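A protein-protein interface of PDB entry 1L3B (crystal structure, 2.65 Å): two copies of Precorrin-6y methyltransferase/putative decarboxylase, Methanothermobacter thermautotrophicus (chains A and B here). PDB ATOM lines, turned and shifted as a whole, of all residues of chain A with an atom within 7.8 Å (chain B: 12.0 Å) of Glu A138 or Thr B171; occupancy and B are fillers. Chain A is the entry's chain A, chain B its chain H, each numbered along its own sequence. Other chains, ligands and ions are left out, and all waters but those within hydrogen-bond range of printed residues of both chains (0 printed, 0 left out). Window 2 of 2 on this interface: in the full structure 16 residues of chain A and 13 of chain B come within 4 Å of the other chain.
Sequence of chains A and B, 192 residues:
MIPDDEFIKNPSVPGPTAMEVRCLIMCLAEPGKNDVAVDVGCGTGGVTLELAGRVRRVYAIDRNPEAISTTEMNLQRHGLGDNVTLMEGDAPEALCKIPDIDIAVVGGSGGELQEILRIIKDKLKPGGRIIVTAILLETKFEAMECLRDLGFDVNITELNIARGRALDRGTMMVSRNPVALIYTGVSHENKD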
ATOM      1  N   SER A 109      28.150  16.086  -2.383  1.00  0.00           N
ATOM      2  CA  SER A 109      27.769  16.006  -3.812  1.00  0.00           C
ATOM      3  C   SER A 109      28.870  15.402  -4.683  1.00  0.00           C
ATOM      4  O   SER A 109      28.691  14.343  -5.288  1.00  0.00           O
ATOM      5  CB  SER A 109      27.443  17.390  -4.379  1.00  0.00           C
ATOM      6  OG  SER A 109      27.666  17.413  -5.788  1.00  0.00           O
ATOM      7  N   LEU A 113      26.463  15.039  -8.428  1.00  0.00           N
ATOM      8  CA  LEU A 113      25.259  14.727  -7.665  1.00  0.00           C
ATOM      9  C   LEU A 113      24.138  14.173  -8.522  1.00  0.00           C
ATOM     10  O   LEU A 113      23.646  13.072  -8.270  1.00  0.00           O
ATOM     11  CB  LEU A 113      24.767  15.969  -6.931  1.00  0.00           C
ATOM     12  CG  LEU A 113      23.439  15.804  -6.207  1.00  0.00           C
ATOM     13  CD1 LEU A 113      23.502  14.647  -5.237  1.00  0.00           C
ATOM     14  CD2 LEU A 113      23.122  17.096  -5.487  1.00  0.00           C
ATOM     15  N   ALA A 134      23.462  17.578   2.755  1.00  0.00           N
ATOM     16  CA  ALA A 134      24.025  18.743   2.072  1.00  0.00           C
ATOM     17  C   ALA A 134      24.447  19.893   2.982  1.00  0.00           C
ATOM     18  O   ALA A 134      23.709  20.304   3.876  1.00  0.00           O
ATOM     19  CB  ALA A 134      23.024  19.254   1.050  1.00  0.00           C
ATOM     20  N   ILE A 135      25.630  20.428   2.725  1.00  0.00           N
ATOM     21  CA  ILE A 135      26.145  21.527   3.513  1.00  0.00           C
ATOM     22  C   ILE A 135      26.223  22.738   2.601  1.00  0.00           C
ATOM     23  O   ILE A 135      26.251  23.882   3.055  1.00  0.00           O
ATOM     24  CB  ILE A 135      27.556  21.196   4.042  1.00  0.00           C
ATOM     25  CG1 ILE A 135      27.466  20.079   5.080  1.00  0.00           C
ATOM     26  CG2 ILE A 135      28.239  22.460   4.554  1.00  0.00           C
ATOM     27  CD1 ILE A 135      26.720  20.450   6.373  1.00  0.00           C
ATOM     28  N   LEU A 136      26.250  22.463   1.302  1.00  0.00           N
ATOM     29  CA  LEU A 136      26.329  23.517   0.310  1.00  0.00           C
ATOM     30  C   LEU A 136      24.950  23.970  -0.138  1.00  0.00           C
ATOM     31  O   LEU A 136      24.065  23.153  -0.386  1.00  0.00           O
ATOM     32  CB  LEU A 136      27.132  23.036  -0.900  1.00  0.00           C
ATOM     33  CG  LEU A 136      28.605  22.687  -0.639  1.00  0.00           C
ATOM     34  CD1 LEU A 136      29.176  22.118  -1.925  1.00  0.00           C
ATOM     35  CD2 LEU A 136      29.403  23.918  -0.191  1.00  0.00           C
ATOM     36  N   LEU A 137      24.775  25.279  -0.242  1.00  0.00           N
ATOM     37  CA  LEU A 137      23.507  25.851  -0.660  1.00  0.00           C
ATOM     38  C   LEU A 137      22.991  25.237  -1.953  1.00  0.00           C
ATOM     39  O   LEU A 137      21.834  24.839  -2.047  1.00  0.00           O
ATOM     40  CB  LEU A 137      23.667  27.356  -0.844  1.00  0.00           C
ATOM     41  CG  LEU A 137      22.417  28.094  -1.300  1.00  0.00           C
ATOM     42  CD1 LEU A 137      21.248  27.757  -0.389  1.00  0.00           C
ATOM     43  CD2 LEU A 137      22.705  29.571  -1.267  1.00  0.00           C
ATOM     44  N   GLU A 138      23.869  25.182  -2.946  1.00  0.00           N
ATOM     45  CA  GLU A 138      23.551  24.631  -4.250  1.00  0.00           C
ATOM     46  C   GLU A 138      23.211  23.129  -4.193  1.00  0.00           C
ATOM     47  O   GLU A 138      22.324  22.644  -4.917  1.00  0.00           O
ATOM     48  CB  GLU A 138      24.723  24.878  -5.195  1.00  0.00           C
ATOM     49  CG  GLU A 138      25.071  26.360  -5.408  1.00  0.00           C
ATOM     50  CD  GLU A 138      25.845  26.999  -4.258  1.00  0.00           C
ATOM     51  OE1 GLU A 138      26.394  26.271  -3.395  1.00  0.00           O
ATOM     52  OE2 GLU A 138      25.923  28.252  -4.220  1.00  0.00           O
ATOM     53  N   THR A 139      23.898  22.379  -3.336  1.00  0.00           N
ATOM     54  CA  THR A 139      23.614  20.950  -3.239  1.00  0.00           C
ATOM     55  C   THR A 139      22.220  20.717  -2.685  1.00  0.00           C
ATOM     56  O   THR A 139      21.563  19.757  -3.059  1.00  0.00           O
ATOM     57  CB  THR A 139      24.616  20.222  -2.339  1.00  0.00           C
ATOM     58  OG1 THR A 139      25.946  20.431  -2.835  1.00  0.00           O
ATOM     59  CG2 THR A 139      24.307  18.735  -2.324  1.00  0.00           C
ATOM     60  N   LYS A 140      21.766  21.591  -1.793  1.00  0.00           N
ATOM     61  CA  LYS A 140      20.442  21.420  -1.231  1.00  0.00           C
ATOM     62  C   LYS A 140      19.416  21.567  -2.339  1.00  0.00           C
ATOM     63  O   LYS A 140      18.558  20.703  -2.523  1.00  0.00           O
ATOM     64  CB  LYS A 140      20.213  22.433  -0.113  1.00  0.00           C
ATOM     65  CG  LYS A 140      21.117  22.166   1.091  1.00  0.00           C
ATOM     66  CD  LYS A 140      20.948  23.199   2.195  1.00  0.00           C
ATOM     67  CE  LYS A 140      22.114  23.154   3.180  1.00  0.00           C
ATOM     68  NZ  LYS A 140      22.184  24.393   4.008  1.00  0.00           N
ATOM     69  N   PHE A 141      19.539  22.643  -3.109  1.00  0.00           N
ATOM     70  CA  PHE A 141      18.618  22.905  -4.214  1.00  0.00           C
ATOM     71  C   PHE A 141      18.648  21.833  -5.297  1.00  0.00           C
ATOM     72  O   PHE A 141      17.606  21.285  -5.663  1.00  0.00           O
ATOM     73  CB  PHE A 141      18.935  24.235  -4.872  1.00  0.00           C
ATOM     74  CG  PHE A 141      18.084  24.519  -6.063  1.00  0.00           C
ATOM     75  CD1 PHE A 141      16.734  24.804  -5.902  1.00  0.00           C
ATOM     76  CD2 PHE A 141      18.621  24.491  -7.347  1.00  0.00           C
ATOM     77  CE1 PHE A 141      15.926  25.060  -6.990  1.00  0.00           C
ATOM     78  CE2 PHE A 141      17.820  24.746  -8.444  1.00  0.00           C
ATOM     79  CZ  PHE A 141      16.463  25.034  -8.265  1.00  0.00           C
ATOM     80  N   GLU A 142      19.840  21.564  -5.830  1.00  0.00           N
ATOM     81  CA  GLU A 142      19.974  20.557  -6.872  1.00  0.00           C
ATOM     82  C   GLU A 142      19.407  19.206  -6.428  1.00  0.00           C
ATOM     83  O   GLU A 142      18.863  18.481  -7.245  1.00  0.00           O
ATOM     84  CB  GLU A 142      21.443  20.423  -7.322  1.00  0.00           C
ATOM     85  CG  GLU A 142      21.769  19.152  -8.161  1.00  0.00           C
ATOM     86  CD  GLU A 142      21.316  19.198  -9.635  1.00  0.00           C
ATOM     87  OE1 GLU A 142      20.122  19.470  -9.896  1.00  0.00           O
ATOM     88  OE2 GLU A 142      22.155  18.932 -10.536  1.00  0.00           O
ATOM     89  N   ALA A 143      19.508  18.871  -5.144  1.00  0.00           N
ATOM     90  CA  ALA A 143      18.982  17.593  -4.664  1.00  0.00           C
ATOM     91  C   ALA A 143      17.463  17.576  -4.755  1.00  0.00           C
ATOM     92  O   ALA A 143      16.872  16.680  -5.356  1.00  0.00           O
ATOM     93  CB  ALA A 143      19.420  17.343  -3.237  1.00  0.00           C
ATOM     94  N   MET A 144      16.837  18.573  -4.143  1.00  0.00           N
ATOM     95  CA  MET A 144      15.382  18.703  -4.148  1.00  0.00           C
ATOM     96  C   MET A 144      14.836  18.556  -5.566  1.00  0.00           C
ATOM     97  O   MET A 144      14.019  17.678  -5.838  1.00  0.00           O
ATOM     98  CB  MET A 144      14.972  20.072  -3.600  1.00  0.00           C
ATOM     99  CG  MET A 144      14.953  20.201  -2.079  1.00  0.00           C
ATOM    100  SD  MET A 144      13.354  19.429  -1.269  1.00  0.00           S
ATOM    101  CE  MET A 144      12.157  20.941  -1.518  1.00  0.00           C
ATOM    102  N   ALA B 162      24.031  32.452  10.052  1.00  0.00           N
ATOM    103  CA  ALA B 162      24.799  31.640   9.113  1.00  0.00           C
ATOM    104  C   ALA B 162      25.126  32.510   7.892  1.00  0.00           C
ATOM    105  O   ALA B 162      24.225  33.034   7.245  1.00  0.00           O
ATOM    106  CB  ALA B 162      24.000  30.452   8.696  1.00  0.00           C
ATOM    107  N   ARG B 163      26.410  32.669   7.583  1.00  0.00           N
ATOM    108  CA  ARG B 163      26.826  33.478   6.445  1.00  0.00           C
ATOM    109  C   ARG B 163      27.344  32.558   5.365  1.00  0.00           C
ATOM    110  O   ARG B 163      27.784  31.447   5.653  1.00  0.00           O
ATOM    111  CB  ARG B 163      27.888  34.473   6.875  1.00  0.00           C
ATOM    112  CG  ARG B 163      27.400  35.412   7.957  1.00  0.00           C
ATOM    113  CD  ARG B 163      28.379  36.541   8.206  1.00  0.00           C
ATOM    114  NE  ARG B 163      29.096  36.358   9.461  1.00  0.00           N
ATOM    115  CZ  ARG B 163      29.505  37.348  10.252  1.00  0.00           C
ATOM    116  NH1 ARG B 163      29.265  38.606   9.916  1.00  0.00           N
ATOM    117  NH2 ARG B 163      30.148  37.077  11.388  1.00  0.00           N
ATOM    118  N   GLY B 164      27.286  33.002   4.118  1.00  0.00           N
ATOM    119  CA  GLY B 164      27.757  32.153   3.045  1.00  0.00           C
ATOM    120  C   GLY B 164      29.238  32.258   2.748  1.00  0.00           C
ATOM    121  O   GLY B 164      29.800  33.346   2.755  1.00  0.00           O
ATOM    122  N   ARG B 165      29.888  31.123   2.515  1.00  0.00           N
ATOM    123  CA  ARG B 165      31.307  31.161   2.210  1.00  0.00           C
ATOM    124  C   ARG B 165      31.528  30.485   0.867  1.00  0.00           C
ATOM    125  O   ARG B 165      31.316  29.283   0.716  1.00  0.00           O
ATOM    126  CB  ARG B 165      32.154  30.472   3.282  1.00  0.00           C
ATOM    127  CG  ARG B 165      33.664  30.638   3.023  1.00  0.00           C
ATOM    128  CD  ARG B 165      34.515  29.739   3.914  1.00  0.00           C
ATOM    129  NE  ARG B 165      34.393  30.085   5.330  1.00  0.00           N
ATOM    130  CZ  ARG B 165      34.826  29.311   6.318  1.00  0.00           C
ATOM    131  NH1 ARG B 165      35.408  28.150   6.037  1.00  0.00           N
ATOM    132  NH2 ARG B 165      34.656  29.680   7.581  1.00  0.00           N
ATOM    133  N   ALA B 166      31.954  31.283  -0.106  1.00  0.00           N
ATOM    134  CA  ALA B 166      32.216  30.807  -1.455  1.00  0.00           C
ATOM    135  C   ALA B 166      33.416  29.880  -1.482  1.00  0.00           C
ATOM    136  O   ALA B 166      34.504  30.232  -1.036  1.00  0.00           O
ATOM    137  CB  ALA B 166      32.452  31.992  -2.393  1.00  0.00           C
ATOM    138  N   LEU B 167      33.192  28.676  -1.981  1.00  0.00           N
ATOM    139  CA  LEU B 167      34.239  27.678  -2.085  1.00  0.00           C
ATOM    140  C   LEU B 167      34.275  27.319  -3.574  1.00  0.00           C
ATOM    141  O   LEU B 167      33.320  27.622  -4.304  1.00  0.00           O
ATOM    142  CB  LEU B 167      33.896  26.452  -1.235  1.00  0.00           C
ATOM    143  CG  LEU B 167      33.837  26.644   0.282  1.00  0.00           C
ATOM    144  CD1 LEU B 167      33.912  25.269   0.947  1.00  0.00           C
ATOM    145  CD2 LEU B 167      35.008  27.521   0.773  1.00  0.00           C
ATOM    146  N   ASP B 168      35.355  26.696  -4.043  1.00  0.00           N
ATOM    147  CA  ASP B 168      35.416  26.343  -5.460  1.00  0.00           C
ATOM    148  C   ASP B 168      34.196  25.483  -5.788  1.00  0.00           C
ATOM    149  O   ASP B 168      33.557  25.661  -6.824  1.00  0.00           O
ATOM    150  CB  ASP B 168      36.712  25.579  -5.795  1.00  0.00           C
ATOM    151  CG  ASP B 168      37.955  26.257  -5.257  1.00  0.00           C
ATOM    152  OD1 ASP B 168      38.213  26.151  -4.033  1.00  0.00           O
ATOM    153  OD2 ASP B 168      38.680  26.899  -6.056  1.00  0.00           O
ATOM    154  N   ARG B 169      33.872  24.580  -4.869  1.00  0.00           N
ATOM    155  CA  ARG B 169      32.751  23.662  -4.994  1.00  0.00           C
ATOM    156  C   ARG B 169      31.373  24.320  -4.911  1.00  0.00           C
ATOM    157  O   ARG B 169      30.398  23.777  -5.435  1.00  0.00           O
ATOM    158  CB  ARG B 169      32.880  22.561  -3.921  1.00  0.00           C
ATOM    159  CG  ARG B 169      34.022  22.797  -2.909  1.00  0.00           C
ATOM    160  CD  ARG B 169      34.411  21.526  -2.144  1.00  0.00           C
ATOM    161  NE  ARG B 169      33.882  21.456  -0.778  1.00  0.00           N
ATOM    162  CZ  ARG B 169      34.463  22.002   0.289  1.00  0.00           C
ATOM    163  NH1 ARG B 169      35.599  22.672   0.165  1.00  0.00           N
ATOM    164  NH2 ARG B 169      33.921  21.857   1.489  1.00  0.00           N
ATOM    165  N   GLY B 170      31.286  25.483  -4.262  1.00  0.00           N
ATOM    166  CA  GLY B 170      30.004  26.167  -4.140  1.00  0.00           C
ATOM    167  C   GLY B 170      29.881  27.079  -2.931  1.00  0.00           C
ATOM    168  O   GLY B 170      30.878  27.588  -2.430  1.00  0.00           O
ATOM    169  N   THR B 171      28.655  27.291  -2.462  1.00  0.00           N
ATOM    170  CA  THR B 171      28.430  28.154  -1.306  1.00  0.00           C
ATOM    171  C   THR B 171      28.124  27.384  -0.039  1.00  0.00           C
ATOM    172  O   THR B 171      27.070  26.760   0.084  1.00  0.00           O
ATOM    173  CB  THR B 171      27.265  29.112  -1.530  1.00  0.00           C
ATOM    174  OG1 THR B 171      27.417  29.765  -2.798  1.00  0.00           O
ATOM    175  CG2 THR B 171      27.232  30.160  -0.421  1.00  0.00           C
ATOM    176  N   MET B 172      29.035  27.456   0.917  1.00  0.00           N
ATOM    177  CA  MET B 172      28.849  26.755   2.176  1.00  0.00           C
ATOM    178  C   MET B 172      28.222  27.597   3.277  1.00  0.00           C
ATOM    179  O   MET B 172      28.589  28.755   3.487  1.00  0.00           O
ATOM    180  CB  MET B 172      30.184  26.230   2.659  1.00  0.00           C
ATOM    181  CG  MET B 172      30.076  25.419   3.919  1.00  0.00           C
ATOM    182  SD  MET B 172      31.811  24.808   4.455  1.00  0.00           S
ATOM    183  CE  MET B 172      32.774  26.481   4.194  1.00  0.00           C
ATOM    184  N   MET B 173      27.270  27.034   4.000  1.00  0.00           N
ATOM    185  CA  MET B 173      26.687  27.853   5.047  1.00  0.00           C
ATOM    186  C   MET B 173      27.484  27.721   6.332  1.00  0.00           C
ATOM    187  O   MET B 173      27.526  26.658   6.964  1.00  0.00           O
ATOM    188  CB  MET B 173      25.208  27.511   5.288  1.00  0.00           C
ATOM    189  CG  MET B 173      24.229  27.821   4.069  1.00  0.00           C
ATOM    190  SD  MET B 173      24.390  29.566   3.167  1.00  0.00           S
ATOM    191  CE  MET B 173      23.598  30.833   4.526  1.00  0.00           C
ATOM    192  N   VAL B 174      28.131  28.808   6.720  1.00  0.00           N
ATOM    193  CA  VAL B 174      28.919  28.766   7.937  1.00  0.00           C
ATOM    194  C   VAL B 174      28.183  29.438   9.082  1.00  0.00           C
ATOM    195  O   VAL B 174      27.843  30.619   9.018  1.00  0.00           O
ATOM    196  CB  VAL B 174      30.315  29.431   7.749  1.00  0.00           C
ATOM    197  CG1 VAL B 174      31.177  29.176   8.979  1.00  0.00           C
ATOM    198  CG2 VAL B 174      31.006  28.858   6.518  1.00  0.00           C
ATOM    199  N   SER B 175      27.978  28.680  10.149  1.00  0.00           N
ATOM    200  CA  SER B 175      27.280  29.174  11.325  1.00  0.00           C
ATOM    201  C   SER B 175      28.091  29.799  12.461  1.00  0.00           C
ATOM    202  O   SER B 175      29.093  29.249  12.898  1.00  0.00           O
ATOM    203  CB  SER B 175      26.446  28.044  11.920  1.00  0.00           C
ATOM    204  OG  SER B 175      25.080  28.449  12.057  1.00  0.00           O
ATOM    205  N   ARG B 176      27.663  30.961  12.938  1.00  0.00           N
ATOM    206  CA  ARG B 176      28.368  31.612  14.040  1.00  0.00           C
ATOM    207  C   ARG B 176      27.700  30.953  15.242  1.00  0.00           C
ATOM    208  O   ARG B 176      26.631  30.376  15.094  1.00  0.00           O
ATOM    209  CB  ARG B 176      28.074  33.117  14.070  1.00  0.00           C
ATOM    210  CG  ARG B 176      28.296  33.830  12.756  1.00  0.00           C
ATOM    211  CD  ARG B 176      29.770  34.038  12.506  1.00  0.00           C
ATOM    212  NE  ARG B 176      30.085  34.365  11.113  1.00  0.00           N
ATOM    213  CZ  ARG B 176      30.152  33.474  10.123  1.00  0.00           C
ATOM    214  NH1 ARG B 176      29.921  32.192  10.360  1.00  0.00           N
ATOM    215  NH2 ARG B 176      30.492  33.852   8.895  1.00  0.00           N
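Hydrophobic or aromatic side chains of chain B within 4 Å of the printed part of chain A: Met B172 and Met B173.
Glu A138 touches just these residues of chain B: Gly B170 and Thr B171. Thr B171 touches just these residues of chain A: Leu A136, Leu A137 and Glu A138. Leu A137 touches just one residue of chain B: Thr B171 (2.8 Å). Thr A139 touches none of the printed residues of chain B. No residue of chain B comes within 4 Å of Phe A141. No residue of chain B comes within 4 Å of Glu A142. Of chain A, only Glu A138 (3.6 Å) comes within 4 Å of Gly B170. Of the printed residues of chain B, Lys A140 touches Met B173. Printed residues of chain A within 4 Å of Met B172: Ile A135 and Leu A136. Printed residues of chain A within 4 Å of Met B173: Ile A135 (3.4 Å) and Lys A140 (3.99 Å). Of the printed residues of chain B, Ile A135 touches Met B172 and Met B173. Arg B176 touches none of the printed residues of chain A. The nearest residue of chain B that does not touch Glu A138 is Arg B169 (5.1 Å). The nearest residue of chain A that does not touch Thr B171 is Ile A135 (4.2 Å).
N of Arg B165 lies within hydrogen-bond range of O of Met B172 (2.9 Å).
Ile A135 touches Met B172 (CG2 to CG, 3.5 Å). Leu A136 touches Thr B171 (CA to O, 3.3 Å). N of Met B172 touches CD2 of Leu A136 (3.7 Å). Gly B170 touches Glu A138. NZ of Lys A140 touches CG of Met B173 (3.99 Å).
O of Ile A135 sits at hydrogen-bond distance from N of Met B173 (3.4 Å). N of Leu A137 is in hydrogen-bond range of O of Thr B171 (2.8 Å). OE2 of Glu A138 is in hydrogen-bond range of OG1 of Thr B171 (2.6 Å).
No position is printed for both chains. Of the 8 pairs that touch across the chains among the printed residues, none has its exchanged pair printed and touching as well.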
